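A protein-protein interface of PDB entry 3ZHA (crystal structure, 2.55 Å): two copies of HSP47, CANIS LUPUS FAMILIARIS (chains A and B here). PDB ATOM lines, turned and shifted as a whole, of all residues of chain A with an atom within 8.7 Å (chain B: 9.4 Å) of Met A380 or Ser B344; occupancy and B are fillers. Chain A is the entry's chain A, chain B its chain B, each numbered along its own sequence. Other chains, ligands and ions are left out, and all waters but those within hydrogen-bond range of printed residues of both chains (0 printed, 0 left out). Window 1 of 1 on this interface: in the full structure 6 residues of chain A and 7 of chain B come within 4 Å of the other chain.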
ATOM      1  N   ASP A 186      -3.825 -37.975  24.726  1.00  0.00           N
ATOM      2  CA  ASP A 186      -2.924 -36.923  24.251  1.00  0.00           C
ATOM      3  C   ASP A 186      -3.666 -35.638  23.909  1.00  0.00           C
ATOM      4  O   ASP A 186      -4.888 -35.592  23.978  1.00  0.00           O
ATOM      5  CB  ASP A 186      -2.020 -37.398  23.094  1.00  0.00           C
ATOM      6  CG  ASP A 186      -2.725 -37.875  21.831  1.00  0.00           C
ATOM      7  OD1 ASP A 186      -3.925 -37.521  21.634  1.00  0.00           O
ATOM      8  OD2 ASP A 186      -2.073 -38.564  21.015  1.00  0.00           O
ATOM      9  N   ASN A 187      -2.929 -34.600  23.561  1.00  0.00           N
ATOM     10  CA  ASN A 187      -3.469 -33.302  23.228  1.00  0.00           C
ATOM     11  C   ASN A 187      -3.662 -33.092  21.751  1.00  0.00           C
ATOM     12  O   ASN A 187      -2.743 -33.324  20.963  1.00  0.00           O
ATOM     13  CB  ASN A 187      -2.627 -32.199  23.862  1.00  0.00           C
ATOM     14  CG  ASN A 187      -2.682 -32.219  25.381  1.00  0.00           C
ATOM     15  OD1 ASN A 187      -3.747 -32.317  26.009  1.00  0.00           O
ATOM     16  ND2 ASN A 187      -1.534 -32.140  25.998  1.00  0.00           N
ATOM     17  N   ARG A 188      -4.890 -32.712  21.373  1.00  0.00           N
ATOM     18  CA  ARG A 188      -5.266 -32.458  19.988  1.00  0.00           C
ATOM     19  C   ARG A 188      -6.057 -31.147  19.906  1.00  0.00           C
ATOM     20  O   ARG A 188      -6.425 -30.579  20.934  1.00  0.00           O
ATOM     21  CB  ARG A 188      -6.113 -33.622  19.409  1.00  0.00           C
ATOM     22  CG  ARG A 188      -5.503 -35.017  19.516  1.00  0.00           C
ATOM     23  CD  ARG A 188      -4.342 -35.209  18.579  1.00  0.00           C
ATOM     24  NE  ARG A 188      -3.698 -36.492  18.829  1.00  0.00           N
ATOM     25  CZ  ARG A 188      -3.760 -37.536  18.018  1.00  0.00           C
ATOM     26  NH1 ARG A 188      -4.410 -37.451  16.869  1.00  0.00           N
ATOM     27  NH2 ARG A 188      -3.142 -38.664  18.335  1.00  0.00           N
ATOM     28  N   GLY A 189      -6.312 -30.693  18.685  1.00  0.00           N
ATOM     29  CA  GLY A 189      -7.104 -29.506  18.424  1.00  0.00           C
ATOM     30  C   GLY A 189      -8.511 -29.895  18.031  1.00  0.00           C
ATOM     31  O   GLY A 189      -8.695 -30.782  17.193  1.00  0.00           O
ATOM     32  N   PHE A 190      -9.513 -29.295  18.682  1.00  0.00           N
ATOM     33  CA  PHE A 190     -10.924 -29.533  18.378  1.00  0.00           C
ATOM     34  C   PHE A 190     -11.430 -28.367  17.553  1.00  0.00           C
ATOM     35  O   PHE A 190     -11.377 -27.224  17.986  1.00  0.00           O
ATOM     36  CB  PHE A 190     -11.778 -29.723  19.644  1.00  0.00           C
ATOM     37  CG  PHE A 190     -13.225 -30.125  19.390  1.00  0.00           C
ATOM     38  CD1 PHE A 190     -14.185 -29.172  19.050  1.00  0.00           C
ATOM     39  CD2 PHE A 190     -13.633 -31.446  19.531  1.00  0.00           C
ATOM     40  CE1 PHE A 190     -15.512 -29.537  18.829  1.00  0.00           C
ATOM     41  CE2 PHE A 190     -14.968 -31.812  19.311  1.00  0.00           C
ATOM     42  CZ  PHE A 190     -15.900 -30.853  18.983  1.00  0.00           C
ATOM     43  N   MET A 191     -11.927 -28.663  16.369  1.00  0.00           N
ATOM     44  CA  MET A 191     -12.429 -27.652  15.461  1.00  0.00           C
ATOM     45  C   MET A 191     -13.902 -27.333  15.731  1.00  0.00           C
ATOM     46  O   MET A 191     -14.800 -28.066  15.304  1.00  0.00           O
ATOM     47  CB  MET A 191     -12.197 -28.075  14.010  1.00  0.00           C
ATOM     48  CG  MET A 191     -10.748 -28.336  13.671  1.00  0.00           C
ATOM     49  SD  MET A 191     -10.667 -29.038  12.000  1.00  0.00           S
ATOM     50  CE  MET A 191     -11.436 -30.633  12.240  1.00  0.00           C
ATOM     51  N   VAL A 192     -14.140 -26.239  16.470  1.00  0.00           N
ATOM     52  CA  VAL A 192     -15.467 -25.748  16.810  1.00  0.00           C
ATOM     53  C   VAL A 192     -16.123 -25.308  15.490  1.00  0.00           C
ATOM     54  O   VAL A 192     -17.273 -25.656  15.218  1.00  0.00           O
ATOM     55  CB  VAL A 192     -15.391 -24.637  17.892  1.00  0.00           C
ATOM     56  CG1 VAL A 192     -16.769 -24.055  18.204  1.00  0.00           C
ATOM     57  CG2 VAL A 192     -14.731 -25.167  19.173  1.00  0.00           C
ATOM     58  N   SER A 195     -12.569 -22.063  11.359  1.00  0.00           N
ATOM     59  CA  SER A 195     -11.783 -20.895  11.768  1.00  0.00           C
ATOM     60  C   SER A 195     -11.510 -20.846  13.274  1.00  0.00           C
ATOM     61  O   SER A 195     -10.696 -20.029  13.715  1.00  0.00           O
ATOM     62  CB  SER A 195     -12.481 -19.609  11.335  1.00  0.00           C
ATOM     63  OG  SER A 195     -12.900 -19.651   9.980  1.00  0.00           O
ATOM     64  N   TYR A 196     -12.176 -21.708  14.055  1.00  0.00           N
ATOM     65  CA  TYR A 196     -12.017 -21.742  15.495  1.00  0.00           C
ATOM     66  C   TYR A 196     -11.614 -23.130  16.026  1.00  0.00           C
ATOM     67  O   TYR A 196     -12.387 -24.085  15.948  1.00  0.00           O
ATOM     68  CB  TYR A 196     -13.282 -21.195  16.182  1.00  0.00           C
ATOM     69  CG  TYR A 196     -13.154 -20.949  17.668  1.00  0.00           C
ATOM     70  CD1 TYR A 196     -11.952 -20.538  18.226  1.00  0.00           C
ATOM     71  CD2 TYR A 196     -14.248 -21.097  18.515  1.00  0.00           C
ATOM     72  CE1 TYR A 196     -11.827 -20.329  19.593  1.00  0.00           C
ATOM     73  CE2 TYR A 196     -14.142 -20.848  19.884  1.00  0.00           C
ATOM     74  CZ  TYR A 196     -12.933 -20.429  20.411  1.00  0.00           C
ATOM     75  OH  TYR A 196     -12.789 -20.176  21.750  1.00  0.00           O
ATOM     76  N   THR A 197     -10.394 -23.216  16.576  1.00  0.00           N
ATOM     77  CA  THR A 197      -9.826 -24.428  17.160  1.00  0.00           C
ATOM     78  C   THR A 197      -9.539 -24.248  18.651  1.00  0.00           C
ATOM     79  O   THR A 197      -8.934 -23.260  19.063  1.00  0.00           O
ATOM     80  CB  THR A 197      -8.591 -24.923  16.367  1.00  0.00           C
ATOM     81  OG1 THR A 197      -8.943 -25.068  14.987  1.00  0.00           O
ATOM     82  CG2 THR A 197      -8.047 -26.253  16.898  1.00  0.00           C
ATOM     83  N   VAL A 198      -9.935 -25.242  19.437  1.00  0.00           N
ATOM     84  CA  VAL A 198      -9.761 -25.294  20.879  1.00  0.00           C
ATOM     85  C   VAL A 198      -8.896 -26.517  21.238  1.00  0.00           C
ATOM     86  O   VAL A 198      -9.104 -27.599  20.699  1.00  0.00           O
ATOM     87  CB  VAL A 198     -11.167 -25.302  21.549  1.00  0.00           C
ATOM     88  CG1 VAL A 198     -11.144 -25.936  22.933  1.00  0.00           C
ATOM     89  CG2 VAL A 198     -11.768 -23.893  21.583  1.00  0.00           C
ATOM     90  N   GLY A 199      -7.918 -26.320  22.115  1.00  0.00           N
ATOM     91  CA  GLY A 199      -7.041 -27.390  22.575  1.00  0.00           C
ATOM     92  C   GLY A 199      -7.752 -28.296  23.560  1.00  0.00           C
ATOM     93  O   GLY A 199      -8.243 -27.835  24.601  1.00  0.00           O
ATOM     94  N   VAL A 200      -7.832 -29.589  23.226  1.00  0.00           N
ATOM     95  CA  VAL A 200      -8.508 -30.614  24.051  1.00  0.00           C
ATOM     96  C   VAL A 200      -7.597 -31.799  24.328  1.00  0.00           C
ATOM     97  O   VAL A 200      -6.573 -31.985  23.664  1.00  0.00           O
ATOM     98  CB  VAL A 200      -9.855 -31.117  23.440  1.00  0.00           C
ATOM     99  CG1 VAL A 200     -10.879 -29.988  23.304  1.00  0.00           C
ATOM    100  CG2 VAL A 200      -9.630 -31.845  22.111  1.00  0.00           C
ATOM    101  N   THR A 201      -7.999 -32.615  25.293  1.00  0.00           N
ATOM    102  CA  THR A 201      -7.341 -33.867  25.592  1.00  0.00           C
ATOM    103  C   THR A 201      -8.173 -34.907  24.852  1.00  0.00           C
ATOM    104  O   THR A 201      -9.402 -34.874  24.930  1.00  0.00           O
ATOM    105  CB  THR A 201      -7.289 -34.115  27.110  1.00  0.00           C
ATOM    106  OG1 THR A 201      -6.471 -33.118  27.731  1.00  0.00           O
ATOM    107  CG2 THR A 201      -6.728 -35.463  27.449  1.00  0.00           C
ATOM    108  N   TYR A 349     -12.832 -40.049  14.186  1.00  0.00           N
ATOM    109  CA  TYR A 349     -12.010 -38.992  14.773  1.00  0.00           C
ATOM    110  C   TYR A 349     -12.882 -37.793  15.127  1.00  0.00           C
ATOM    111  O   TYR A 349     -13.134 -36.915  14.291  1.00  0.00           O
ATOM    112  CB  TYR A 349     -10.882 -38.642  13.799  1.00  0.00           C
ATOM    113  CG  TYR A 349      -9.733 -37.887  14.402  1.00  0.00           C
ATOM    114  CD1 TYR A 349      -8.745 -38.548  15.125  1.00  0.00           C
ATOM    115  CD2 TYR A 349      -9.579 -36.517  14.183  1.00  0.00           C
ATOM    116  CE1 TYR A 349      -7.648 -37.860  15.651  1.00  0.00           C
ATOM    117  CE2 TYR A 349      -8.469 -35.823  14.675  1.00  0.00           C
ATOM    118  CZ  TYR A 349      -7.510 -36.498  15.419  1.00  0.00           C
ATOM    119  OH  TYR A 349      -6.426 -35.809  15.910  1.00  0.00           O
ATOM    120  N   ARG A 374     -18.858 -27.125  21.647  1.00  0.00           N
ATOM    121  CA  ARG A 374     -17.740 -26.363  22.175  1.00  0.00           C
ATOM    122  C   ARG A 374     -17.227 -26.971  23.489  1.00  0.00           C
ATOM    123  O   ARG A 374     -17.801 -26.731  24.557  1.00  0.00           O
ATOM    124  CB  ARG A 374     -18.130 -24.861  22.308  1.00  0.00           C
ATOM    125  CG  ARG A 374     -17.207 -23.960  23.141  1.00  0.00           C
ATOM    126  CD  ARG A 374     -16.011 -23.468  22.363  1.00  0.00           C
ATOM    127  NE  ARG A 374     -15.394 -22.295  22.986  1.00  0.00           N
ATOM    128  CZ  ARG A 374     -14.425 -22.340  23.904  1.00  0.00           C
ATOM    129  NH1 ARG A 374     -13.972 -23.509  24.351  1.00  0.00           N
ATOM    130  NH2 ARG A 374     -13.916 -21.218  24.395  1.00  0.00           N
ATOM    131  N   GLY A 377     -11.626 -25.542  26.937  1.00  0.00           N
ATOM    132  CA  GLY A 377     -10.244 -25.450  26.504  1.00  0.00           C
ATOM    133  C   GLY A 377      -9.958 -24.106  25.890  1.00  0.00           C
ATOM    134  O   GLY A 377     -10.882 -23.335  25.600  1.00  0.00           O
ATOM    135  N   ASP A 378      -8.668 -23.810  25.706  1.00  0.00           N
ATOM    136  CA  ASP A 378      -8.235 -22.526  25.173  1.00  0.00           C
ATOM    137  C   ASP A 378      -8.145 -22.526  23.654  1.00  0.00           C
ATOM    138  O   ASP A 378      -7.773 -23.539  23.053  1.00  0.00           O
ATOM    139  CB  ASP A 378      -6.902 -22.081  25.818  1.00  0.00           C
ATOM    140  CG  ASP A 378      -6.892 -22.014  27.342  1.00  0.00           C
ATOM    141  OD1 ASP A 378      -7.936 -21.658  27.932  1.00  0.00           O
ATOM    142  OD2 ASP A 378      -5.820 -22.271  27.941  1.00  0.00           O
ATOM    143  N   LYS A 379      -8.495 -21.372  23.041  1.00  0.00           N
ATOM    144  CA  LYS A 379      -8.428 -21.143  21.599  1.00  0.00           C
ATOM    145  C   LYS A 379      -6.964 -21.251  21.128  1.00  0.00           C
ATOM    146  O   LYS A 379      -6.073 -20.691  21.757  1.00  0.00           O
ATOM    147  CB  LYS A 379      -9.020 -19.764  21.227  1.00  0.00           C
ATOM    148  CG  LYS A 379      -8.920 -19.454  19.727  1.00  0.00           C
ATOM    149  CD  LYS A 379      -9.343 -18.048  19.330  1.00  0.00           C
ATOM    150  CE  LYS A 379      -9.358 -17.906  17.823  1.00  0.00           C
ATOM    151  NZ  LYS A 379      -9.787 -16.549  17.397  1.00  0.00           N
ATOM    152  N   MET A 380      -6.741 -21.989  20.038  1.00  0.00           N
ATOM    153  CA  MET A 380      -5.441 -22.198  19.412  1.00  0.00           C
ATOM    154  C   MET A 380      -5.366 -21.391  18.130  1.00  0.00           C
ATOM    155  O   MET A 380      -6.366 -20.826  17.682  1.00  0.00           O
ATOM    156  CB  MET A 380      -5.288 -23.669  19.027  1.00  0.00           C
ATOM    157  CG  MET A 380      -4.953 -24.562  20.159  1.00  0.00           C
ATOM    158  SD  MET A 380      -4.930 -26.299  19.648  1.00  0.00           S
ATOM    159  CE  MET A 380      -3.804 -26.927  20.917  1.00  0.00           C
ATOM    160  N   ARG A 381      -4.198 -21.388  17.508  1.00  0.00           N
ATOM    161  CA  ARG A 381      -4.001 -20.771  16.222  1.00  0.00           C
ATOM    162  C   ARG A 381      -3.618 -21.919  15.278  1.00  0.00           C
ATOM    163  O   ARG A 381      -2.632 -22.627  15.532  1.00  0.00           O
ATOM    164  CB  ARG A 381      -2.891 -19.724  16.302  1.00  0.00           C
ATOM    165  N   ASP A 382      -4.469 -22.172  14.260  1.00  0.00           N
ATOM    166  CA  ASP A 382      -4.181 -23.163  13.229  1.00  0.00           C
ATOM    167  C   ASP A 382      -3.186 -22.432  12.313  1.00  0.00           C
ATOM    168  O   ASP A 382      -3.570 -21.529  11.552  1.00  0.00           O
ATOM    169  CB  ASP A 382      -5.448 -23.540  12.473  1.00  0.00           C
ATOM    170  N   GLU A 383      -1.875 -22.718  12.522  1.00  0.00           N
ATOM    171  CA  GLU A 383      -0.755 -22.089  11.811  1.00  0.00           C
ATOM    172  C   GLU A 383      -0.938 -22.115  10.282  1.00  0.00           C
ATOM    173  O   GLU A 383      -0.701 -21.109   9.618  1.00  0.00           O
ATOM    174  CB  GLU A 383       0.556 -22.750  12.213  1.00  0.00           C
ATOM    175  N   LEU A 385      -3.887 -22.314   8.622  1.00  0.00           N
ATOM    176  CA  LEU A 385      -5.187 -21.720   8.216  1.00  0.00           C
ATOM    177  C   LEU A 385      -5.019 -20.447   7.364  1.00  0.00           C
ATOM    178  O   LEU A 385      -4.143 -19.610   7.649  1.00  0.00           O
ATOM    179  CB  LEU A 385      -6.070 -21.439   9.430  1.00  0.00           C
ATOM    180  N   THR B 206       5.993 -38.045  15.244  1.00  0.00           N
ATOM    181  CA  THR B 206       5.611 -36.967  16.154  1.00  0.00           C
ATOM    182  C   THR B 206       6.659 -36.960  17.277  1.00  0.00           C
ATOM    183  O   THR B 206       6.934 -37.998  17.886  1.00  0.00           O
ATOM    184  CB  THR B 206       4.157 -37.092  16.661  1.00  0.00           C
ATOM    185  OG1 THR B 206       3.260 -37.081  15.556  1.00  0.00           O
ATOM    186  CG2 THR B 206       3.767 -35.970  17.598  1.00  0.00           C
ATOM    187  N   GLY B 207       7.241 -35.795  17.513  1.00  0.00           N
ATOM    188  CA  GLY B 207       8.230 -35.615  18.563  1.00  0.00           C
ATOM    189  C   GLY B 207       8.439 -34.168  18.948  1.00  0.00           C
ATOM    190  O   GLY B 207       7.794 -33.273  18.395  1.00  0.00           O
ATOM    191  N   LEU B 208       9.359 -33.938  19.888  1.00  0.00           N
ATOM    192  CA  LEU B 208       9.736 -32.609  20.357  1.00  0.00           C
ATOM    193  C   LEU B 208      10.864 -32.079  19.479  1.00  0.00           C
ATOM    194  O   LEU B 208      11.934 -32.694  19.388  1.00  0.00           O
ATOM    195  CB  LEU B 208      10.174 -32.652  21.832  1.00  0.00           C
ATOM    196  CG  LEU B 208       9.283 -31.968  22.858  1.00  0.00           C
ATOM    197  CD1 LEU B 208       7.790 -32.391  22.737  1.00  0.00           C
ATOM    198  CD2 LEU B 208       9.796 -32.232  24.263  1.00  0.00           C
ATOM    199  N   TYR B 211      11.142 -25.499  16.619  1.00  0.00           N
ATOM    200  CA  TYR B 211      10.237 -25.106  15.566  1.00  0.00           C
ATOM    201  C   TYR B 211       9.881 -23.633  15.655  1.00  0.00           C
ATOM    202  O   TYR B 211       9.857 -23.050  16.733  1.00  0.00           O
ATOM    203  CB  TYR B 211       8.980 -25.985  15.697  1.00  0.00           C
ATOM    204  CG  TYR B 211       7.858 -25.704  14.724  1.00  0.00           C
ATOM    205  CD1 TYR B 211       7.793 -26.360  13.501  1.00  0.00           C
ATOM    206  CD2 TYR B 211       6.821 -24.840  15.057  1.00  0.00           C
ATOM    207  CE1 TYR B 211       6.741 -26.135  12.618  1.00  0.00           C
ATOM    208  CE2 TYR B 211       5.793 -24.572  14.166  1.00  0.00           C
ATOM    209  CZ  TYR B 211       5.754 -25.224  12.943  1.00  0.00           C
ATOM    210  OH  TYR B 211       4.731 -24.981  12.059  1.00  0.00           O
ATOM    211  N   GLU B 215       4.085 -16.336  10.712  1.00  0.00           N
ATOM    212  CA  GLU B 215       2.736 -16.059  10.200  1.00  0.00           C
ATOM    213  C   GLU B 215       2.754 -14.987   9.116  1.00  0.00           C
ATOM    214  O   GLU B 215       1.928 -15.021   8.188  1.00  0.00           O
ATOM    215  CB  GLU B 215       1.788 -15.617  11.337  1.00  0.00           C
ATOM    216  CG  GLU B 215       1.300 -16.757  12.223  1.00  0.00           C
ATOM    217  CD  GLU B 215       0.539 -17.889  11.548  1.00  0.00           C
ATOM    218  OE1 GLU B 215      -0.317 -17.615  10.675  1.00  0.00           O
ATOM    219  OE2 GLU B 215       0.780 -19.055  11.926  1.00  0.00           O
ATOM    220  N   LYS B 266       8.834 -27.668  20.505  1.00  0.00           N
ATOM    221  CA  LYS B 266       7.396 -27.919  20.475  1.00  0.00           C
ATOM    222  C   LYS B 266       7.165 -29.334  19.974  1.00  0.00           C
ATOM    223  O   LYS B 266       8.041 -29.909  19.316  1.00  0.00           O
ATOM    224  CB  LYS B 266       6.707 -26.950  19.473  1.00  0.00           C
ATOM    225  CG  LYS B 266       6.750 -25.501  19.851  1.00  0.00           C
ATOM    226  CD  LYS B 266       5.797 -24.698  19.009  1.00  0.00           C
ATOM    227  CE  LYS B 266       5.831 -23.238  19.376  1.00  0.00           C
ATOM    228  NZ  LYS B 266       6.996 -22.556  18.744  1.00  0.00           N
ATOM    229  N   ALA B 267       5.948 -29.854  20.209  1.00  0.00           N
ATOM    230  CA  ALA B 267       5.512 -31.112  19.637  1.00  0.00           C
ATOM    231  C   ALA B 267       5.253 -30.818  18.147  1.00  0.00           C
ATOM    232  O   ALA B 267       4.542 -29.860  17.805  1.00  0.00           O
ATOM    233  CB  ALA B 267       4.235 -31.565  20.296  1.00  0.00           C
ATOM    234  N   VAL B 268       5.931 -31.567  17.272  1.00  0.00           N
ATOM    235  CA  VAL B 268       5.816 -31.400  15.825  1.00  0.00           C
ATOM    236  C   VAL B 268       5.554 -32.774  15.194  1.00  0.00           C
ATOM    237  O   VAL B 268       6.248 -33.744  15.521  1.00  0.00           O
ATOM    238  CB  VAL B 268       7.057 -30.683  15.174  1.00  0.00           C
ATOM    239  CG1 VAL B 268       6.840 -30.434  13.681  1.00  0.00           C
ATOM    240  CG2 VAL B 268       7.398 -29.369  15.883  1.00  0.00           C
ATOM    241  N   ALA B 269       4.561 -32.841  14.281  1.00  0.00           N
ATOM    242  CA  ALA B 269       4.245 -34.032  13.517  1.00  0.00           C
ATOM    243  C   ALA B 269       4.906 -33.838  12.151  1.00  0.00           C
ATOM    244  O   ALA B 269       4.471 -33.025  11.336  1.00  0.00           O
ATOM    245  CB  ALA B 269       2.737 -34.210  13.397  1.00  0.00           C
ATOM    246  N   ARG B 343       1.806 -31.206  24.128  1.00  0.00           N
ATOM    247  CA  ARG B 343       0.920 -30.210  23.485  1.00  0.00           C
ATOM    248  C   ARG B 343       0.543 -30.594  22.036  1.00  0.00           C
ATOM    249  O   ARG B 343       1.292 -31.315  21.396  1.00  0.00           O
ATOM    250  CB  ARG B 343       1.533 -28.814  23.537  1.00  0.00           C
ATOM    251  N   SER B 344      -0.638 -30.163  21.554  1.00  0.00           N
ATOM    252  CA  SER B 344      -1.192 -30.490  20.232  1.00  0.00           C
ATOM    253  C   SER B 344      -0.155 -30.230  19.161  1.00  0.00           C
ATOM    254  O   SER B 344       0.354 -29.100  19.102  1.00  0.00           O
ATOM    255  CB  SER B 344      -2.517 -29.763  20.021  1.00  0.00           C
ATOM    256  OG  SER B 344      -2.693 -29.203  18.735  1.00  0.00           O
ATOM    257  N   PRO B 345       0.323 -31.264  18.417  1.00  0.00           N
ATOM    258  CA  PRO B 345       1.445 -30.999  17.519  1.00  0.00           C
ATOM    259  C   PRO B 345       1.183 -30.125  16.326  1.00  0.00           C
ATOM    260  O   PRO B 345       0.096 -30.089  15.755  1.00  0.00           O
ATOM    261  CB  PRO B 345       1.968 -32.386  17.117  1.00  0.00           C
ATOM    262  CG  PRO B 345       0.800 -33.265  17.209  1.00  0.00           C
ATOM    263  CD  PRO B 345      -0.064 -32.695  18.369  1.00  0.00           C
ATOM    264  N   LYS B 346       2.226 -29.399  15.968  1.00  0.00           N
ATOM    265  CA  LYS B 346       2.298 -28.568  14.780  1.00  0.00           C
ATOM    266  C   LYS B 346       2.583 -29.527  13.646  1.00  0.00           C
ATOM    267  O   LYS B 346       3.228 -30.555  13.853  1.00  0.00           O
ATOM    268  CB  LYS B 346       3.455 -27.566  14.882  1.00  0.00           C
ATOM    269  CG  LYS B 346       3.433 -26.699  16.137  1.00  0.00           C
ATOM    270  CD  LYS B 346       2.286 -25.699  16.157  1.00  0.00           C
ATOM    271  CE  LYS B 346       2.108 -25.112  17.533  1.00  0.00           C
ATOM    272  NZ  LYS B 346       0.735 -25.372  18.046  1.00  0.00           N
ATOM    273  N   LEU B 347       2.106 -29.221  12.458  1.00  0.00           N
ATOM    274  CA  LEU B 347       2.354 -30.090  11.317  1.00  0.00           C
ATOM    275  C   LEU B 347       3.514 -29.557  10.517  1.00  0.00           C
ATOM    276  O   LEU B 347       3.541 -28.367  10.178  1.00  0.00           O
ATOM    277  CB  LEU B 347       1.117 -30.171  10.399  1.00  0.00           C
ATOM    278  CG  LEU B 347      -0.187 -30.730  10.992  1.00  0.00           C
ATOM    279  CD1 LEU B 347      -1.280 -30.706   9.951  1.00  0.00           C
ATOM    280  CD2 LEU B 347      -0.010 -32.182  11.554  1.00  0.00           C
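The backbone carbonyl oxygen of Glu A383 sits close to the side-chain carboxylate of Glu B215. SD of Met A380 lies close to OG of Ser B344, 3.8 Å away.
The side-chain hydroxyl (OH) of Tyr A349 lies within hydrogen-bond range of the guanidinium group (NH1) of Arg A188. The side-chain carboxylate (OD2) of Asp A186 is in salt-bridge range of the guanidinium group (NH2) of Arg A188. O of Arg A188 is in hydrogen-bond range of N of Val A200, 2.9 Å away. The backbone NH of Met A380 sits at hydrogen-bond distance from the backbone carbonyl oxygen of Thr A197, at 2.7 Å. OD1 of Asn A187 is in hydrogen-bond range of OG1 of Thr A201, 3.3 Å away.
Asn A187 touches Arg B343 (ND2 to N, 3.9 Å). O of Asn A187 touches CA of Ser B344, 3.3 Å away. O of Asn A187 touches CD of Pro B345 (3.8 Å). Ser B344 touches Arg A188. Gly A189 touches Ser B344.
Met A380 touches one residue of chain B. Of chain A, only Asn A187, Arg A188, Gly A189 and Met A380 come within 4 Å of Ser B344. No residue of chain B comes within 4 Å of Arg A381. Of the printed residues of chain A, Pro B345 touches Asn A187. Printed residues of chain A within 4 Å of Glu B215: Glu A383. Of the printed residues of chain B, Gly A189 touches Ser B344. Printed residues of chain B within 4 Å of Asn A187: Arg B343 (3.9 Å), Ser B344 (3.3 Å) and Pro B345 (3.8 Å). Thr A201 touches none of the printed residues of chain B. The nearest printed residue of chain B that does not touch Asn A187 is Ala B267 (7.2 Å).
Printed residues of chain A that touch a printed residue of chain B: Asn A187, Arg A188, Gly A189, Met A380 and Glu A383. Hydrophobic or aromatic side chains of chain A within 4 Å of the printed part of chain B: Met A380. Of the 14 printed residues of chain B, 4 touch a printed residue of chain A. Hydrophobic or aromatic side chains of chain B within 4 Å of the printed part of chain A: Pro B345. Along chain B the printed residues that touch a printed residue of chain A span positions 215 to 345. Among the printed residues, no Asp or Glu carboxylate lies within 4 Å of a Lys or Arg side-chain nitrogen of the other chain.
No position is printed for both chains.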
